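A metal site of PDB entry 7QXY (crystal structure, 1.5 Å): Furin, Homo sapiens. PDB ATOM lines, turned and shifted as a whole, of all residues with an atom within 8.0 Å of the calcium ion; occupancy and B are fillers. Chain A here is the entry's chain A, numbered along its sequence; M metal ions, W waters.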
ATOM      1  N   LYS A  51     -39.753 -12.018 -13.456  1.00  0.00           N
ATOM      2  CA  LYS A  51     -39.996 -13.221 -12.660  1.00  0.00           C
ATOM      3  C   LYS A  51     -41.247 -13.164 -11.790  1.00  0.00           C
ATOM      4  O   LYS A  51     -41.765 -14.215 -11.421  1.00  0.00           O
ATOM      5  CB  LYS A  51     -38.764 -13.559 -11.830  1.00  0.00           C
ATOM      6  CG  LYS A  51     -38.460 -12.612 -10.687  1.00  0.00           C
ATOM      7  CD  LYS A  51     -37.068 -12.898 -10.120  1.00  0.00           C
ATOM      8  CE  LYS A  51     -36.737 -11.960  -8.990  1.00  0.00           C
ATOM      9  NZ  LYS A  51     -36.420 -10.594  -9.491  1.00  0.00           N
ATOM     10  N   PHE A  66     -29.862 -15.968 -14.652  1.00  0.00           N
ATOM     11  CA  PHE A  66     -28.686 -15.211 -14.243  1.00  0.00           C
ATOM     12  C   PHE A  66     -28.692 -13.865 -14.959  1.00  0.00           C
ATOM     13  O   PHE A  66     -29.365 -13.709 -15.973  1.00  0.00           O
ATOM     14  CB  PHE A  66     -27.354 -15.959 -14.554  1.00  0.00           C
ATOM     15  CG  PHE A  66     -26.221 -15.553 -13.622  1.00  0.00           C
ATOM     16  CD1 PHE A  66     -26.173 -16.043 -12.328  1.00  0.00           C
ATOM     17  CD2 PHE A  66     -25.250 -14.661 -14.026  1.00  0.00           C
ATOM     18  CE1 PHE A  66     -25.168 -15.629 -11.452  1.00  0.00           C
ATOM     19  CE2 PHE A  66     -24.259 -14.250 -13.145  1.00  0.00           C
ATOM     20  CZ  PHE A  66     -24.218 -14.735 -11.869  1.00  0.00           C
ATOM     21  N   ASP A  67     -27.981 -12.902 -14.410  1.00  0.00           N
ATOM     22  CA  ASP A  67     -27.841 -11.598 -15.019  1.00  0.00           C
ATOM     23  C   ASP A  67     -26.379 -11.413 -15.357  1.00  0.00           C
ATOM     24  O   ASP A  67     -25.569 -11.051 -14.490  1.00  0.00           O
ATOM     25  CB  ASP A  67     -28.346 -10.499 -14.083  1.00  0.00           C
ATOM     26  CG  ASP A  67     -28.233  -9.089 -14.622  1.00  0.00           C
ATOM     27  OD1 ASP A  67     -27.533  -8.888 -15.638  1.00  0.00           O
ATOM     28  OD2 ASP A  67     -28.814  -8.179 -13.997  1.00  0.00           O
ATOM     29  N   VAL A  68     -26.044 -11.662 -16.602  1.00  0.00           N
ATOM     30  CA  VAL A  68     -24.671 -11.546 -17.062  1.00  0.00           C
ATOM     31  C   VAL A  68     -24.296 -10.105 -17.382  1.00  0.00           C
ATOM     32  O   VAL A  68     -23.105  -9.801 -17.404  1.00  0.00           O
ATOM     33  CB  VAL A  68     -24.447 -12.522 -18.252  1.00  0.00           C
ATOM     34  CG1 VAL A  68     -23.044 -12.386 -18.787  1.00  0.00           C
ATOM     35  CG2 VAL A  68     -24.711 -13.961 -17.800  1.00  0.00           C
ATOM     36  N   ASN A  69     -25.272  -9.195 -17.622  1.00  0.00           N
ATOM     37  CA  ASN A  69     -24.954  -7.793 -17.884  1.00  0.00           C
ATOM     38  C   ASN A  69     -24.490  -7.064 -16.624  1.00  0.00           C
ATOM     39  O   ASN A  69     -23.551  -6.267 -16.683  1.00  0.00           O
ATOM     40  CB  ASN A  69     -26.144  -7.083 -18.502  1.00  0.00           C
ATOM     41  CG  ASN A  69     -26.502  -7.612 -19.870  1.00  0.00           C
ATOM     42  OD1 ASN A  69     -27.682  -7.866 -20.162  1.00  0.00           O
ATOM     43  ND2 ASN A  69     -25.527  -7.723 -20.783  1.00  0.00           N
ATOM     44  N   ASP A  70     -25.133  -7.337 -15.483  1.00  0.00           N
ATOM     45  CA  ASP A  70     -24.777  -6.713 -14.204  1.00  0.00           C
ATOM     46  C   ASP A  70     -24.038  -7.659 -13.255  1.00  0.00           C
ATOM     47  O   ASP A  70     -23.695  -7.247 -12.151  1.00  0.00           O
ATOM     48  CB  ASP A  70     -26.038  -6.138 -13.508  1.00  0.00           C
ATOM     49  CG  ASP A  70     -26.529  -4.814 -14.085  1.00  0.00           C
ATOM     50  OD1 ASP A  70     -25.808  -4.213 -14.917  1.00  0.00           O
ATOM     51  OD2 ASP A  70     -27.644  -4.388 -13.727  1.00  0.00           O
ATOM     52  N   GLN A  71     -23.792  -8.921 -13.646  1.00  0.00           N
ATOM     53  CA  GLN A  71     -23.045  -9.862 -12.833  1.00  0.00           C
ATOM     54  C   GLN A  71     -23.730 -10.120 -11.494  1.00  0.00           C
ATOM     55  O   GLN A  71     -23.157  -9.896 -10.440  1.00  0.00           O
ATOM     56  CB  GLN A  71     -21.573  -9.407 -12.703  1.00  0.00           C
ATOM     57  CG  GLN A  71     -20.971  -9.139 -14.094  1.00  0.00           C
ATOM     58  CD  GLN A  71     -19.460  -9.117 -14.124  1.00  0.00           C
ATOM     59  OE1 GLN A  71     -18.813  -8.486 -13.283  1.00  0.00           O
ATOM     60  NE2 GLN A  71     -18.864  -9.779 -15.097  1.00  0.00           N
ATOM     61  N   ASP A  72     -24.981 -10.590 -11.552  1.00  0.00           N
ATOM     62  CA  ASP A  72     -25.751 -10.948 -10.356  1.00  0.00           C
ATOM     63  C   ASP A  72     -26.744 -12.062 -10.702  1.00  0.00           C
ATOM     64  O   ASP A  72     -26.941 -12.330 -11.887  1.00  0.00           O
ATOM     65  CB  ASP A  72     -26.450  -9.713  -9.740  1.00  0.00           C
ATOM     66  CG  ASP A  72     -27.576  -9.113 -10.576  1.00  0.00           C
ATOM     67  OD1 ASP A  72     -28.586  -9.803 -10.784  1.00  0.00           O
ATOM     68  OD2 ASP A  72     -27.467  -7.930 -10.968  1.00  0.00           O
ATOM     69  N   PRO A  73     -27.390 -12.749  -9.743  1.00  0.00           N
ATOM     70  CA  PRO A  73     -28.297 -13.857 -10.100  1.00  0.00           C
ATOM     71  C   PRO A  73     -29.675 -13.472 -10.595  1.00  0.00           C
ATOM     72  O   PRO A  73     -30.409 -14.365 -11.018  1.00  0.00           O
ATOM     73  CB  PRO A  73     -28.508 -14.583  -8.755  1.00  0.00           C
ATOM     74  CG  PRO A  73     -27.417 -14.114  -7.912  1.00  0.00           C
ATOM     75  CD  PRO A  73     -27.251 -12.678  -8.280  1.00  0.00           C
ATOM     76  N   ASP A  74     -30.078 -12.208 -10.415  1.00  0.00           N
ATOM     77  CA  ASP A  74     -31.438 -11.723 -10.661  1.00  0.00           C
ATOM     78  C   ASP A  74     -31.608 -11.134 -12.058  1.00  0.00           C
ATOM     79  O   ASP A  74     -31.089 -10.048 -12.331  1.00  0.00           O
ATOM     80  CB  ASP A  74     -31.765 -10.689  -9.581  1.00  0.00           C
ATOM     81  CG  ASP A  74     -33.177 -10.131  -9.635  1.00  0.00           C
ATOM     82  OD1 ASP A  74     -33.929 -10.481 -10.567  1.00  0.00           O
ATOM     83  OD2 ASP A  74     -33.529  -9.337  -8.733  1.00  0.00           O
ATOM     84  N   PRO A  75     -32.344 -11.828 -12.955  1.00  0.00           N
ATOM     85  CA  PRO A  75     -32.484 -11.351 -14.335  1.00  0.00           C
ATOM     86  C   PRO A  75     -33.634 -10.377 -14.545  1.00  0.00           C
ATOM     87  O   PRO A  75     -34.096 -10.222 -15.689  1.00  0.00           O
ATOM     88  CB  PRO A  75     -32.794 -12.653 -15.082  1.00  0.00           C
ATOM     89  CG  PRO A  75     -33.728 -13.330 -14.135  1.00  0.00           C
ATOM     90  CD  PRO A  75     -33.052 -13.119 -12.773  1.00  0.00           C
ATOM     91  N   GLN A  76     -34.117  -9.705 -13.472  1.00  0.00           N
ATOM     92  CA  GLN A  76     -35.249  -8.778 -13.634  1.00  0.00           C
ATOM     93  C   GLN A  76     -34.922  -7.722 -14.730  1.00  0.00           C
ATOM     94  O   GLN A  76     -33.795  -7.210 -14.722  1.00  0.00           O
ATOM     95  CB  GLN A  76     -35.525  -8.043 -12.312  1.00  0.00           C
ATOM     96  CG  GLN A  76     -36.873  -7.284 -12.279  1.00  0.00           C
ATOM     97  CD  GLN A  76     -38.078  -8.197 -12.160  1.00  0.00           C
ATOM     98  OE1 GLN A  76     -37.982  -9.368 -11.806  1.00  0.00           O
ATOM     99  NE2 GLN A  76     -39.257  -7.666 -12.437  1.00  0.00           N
ATOM    100  N   PRO A  77     -35.818  -7.434 -15.677  1.00  0.00           N
ATOM    101  CA  PRO A  77     -35.493  -6.433 -16.697  1.00  0.00           C
ATOM    102  C   PRO A  77     -35.306  -5.036 -16.120  1.00  0.00           C
ATOM    103  O   PRO A  77     -35.835  -4.701 -15.052  1.00  0.00           O
ATOM    104  CB  PRO A  77     -36.702  -6.446 -17.640  1.00  0.00           C
ATOM    105  CG  PRO A  77     -37.462  -7.667 -17.310  1.00  0.00           C
ATOM    106  CD  PRO A  77     -37.176  -7.987 -15.887  1.00  0.00           C
ATOM    107  N   ARG A  78     -34.600  -4.199 -16.881  1.00  0.00           N
ATOM    108  CA  ARG A  78     -34.435  -2.781 -16.534  1.00  0.00           C
ATOM    109  C   ARG A  78     -35.671  -2.069 -17.112  1.00  0.00           C
ATOM    110  O   ARG A  78     -35.925  -2.165 -18.323  1.00  0.00           O
ATOM    111  CB  ARG A  78     -33.147  -2.271 -17.190  1.00  0.00           C
ATOM    112  CG  ARG A  78     -32.794  -0.809 -16.954  1.00  0.00           C
ATOM    113  CD  ARG A  78     -31.408  -0.508 -17.510  1.00  0.00           C
ATOM    114  NE  ARG A  78     -31.334  -0.786 -18.953  1.00  0.00           N
ATOM    115  CZ  ARG A  78     -31.650   0.064 -19.932  1.00  0.00           C
ATOM    116  NH1 ARG A  78     -31.579  -0.323 -21.200  1.00  0.00           N
ATOM    117  NH2 ARG A  78     -32.038   1.301 -19.642  1.00  0.00           N
ATOM    118  N   ARG A 118     -30.269 -12.483 -18.425  1.00  0.00           N
ATOM    119  CA  ARG A 118     -30.269 -11.102 -18.870  1.00  0.00           C
ATOM    120  C   ARG A 118     -28.881 -10.907 -19.440  1.00  0.00           C
ATOM    121  O   ARG A 118     -27.914 -10.835 -18.693  1.00  0.00           O
ATOM    122  CB  ARG A 118     -30.570 -10.131 -17.705  1.00  0.00           C
ATOM    123  CG  ARG A 118     -30.409  -8.651 -18.049  1.00  0.00           C
ATOM    124  CD  ARG A 118     -31.026  -7.778 -16.931  1.00  0.00           C
ATOM    125  NE  ARG A 118     -30.897  -6.360 -17.266  1.00  0.00           N
ATOM    126  CZ  ARG A 118     -29.967  -5.507 -16.822  1.00  0.00           C
ATOM    127  NH1 ARG A 118     -29.949  -4.254 -17.248  1.00  0.00           N
ATOM    128  NH2 ARG A 118     -29.057  -5.903 -15.938  1.00  0.00           N
HETATM  129 CA    CA M   1     -29.822  -8.021 -11.966  1.00  0.00          CA
HETATM  130  O   HOH W   1     -30.695  -7.372  -9.854  1.00  0.00           O
HETATM  131  O   HOH W   2     -31.798  -7.121 -12.737  1.00  0.00           O
HETATM  132  O   HOH W   3     -29.281  -5.727 -12.047  1.00  0.00           O
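Of the 15 residues printed, 3 come within 4 Å of the calcium ion.
The calcium ion is bound by the side-chain carboxylate (OD2) of Asp 67, water W2, water W3, water W1, the backbone carbonyl oxygen (O) of Asp 74, the side-chain carboxylate (OD1) of Asp 72 and the side-chain carboxylate (OD2) of Asp 72. The calcium ion has seven donor atoms within binding distance.
OD1 of Asp 67 sits at hydrogen-bond distance from N of Asp 70 (2.9 Å). NH2 of Arg 118 is in salt-bridge range of OD1 of Asp 67 (3.4 Å). The side-chain carboxylate (OD1) of Asp 67 sits at hydrogen-bond distance from the backbone NH (N) of Asn 69 (3.0 Å). The side-chain carboxylate of Asp 74 is in hydrogen-bond range of the backbone NH of Gln 76 (3.0 Å). The side-chain carboxylate of Asp 74 is in salt-bridge range of the side-chain amino group of Lys 51 (2.7 Å).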
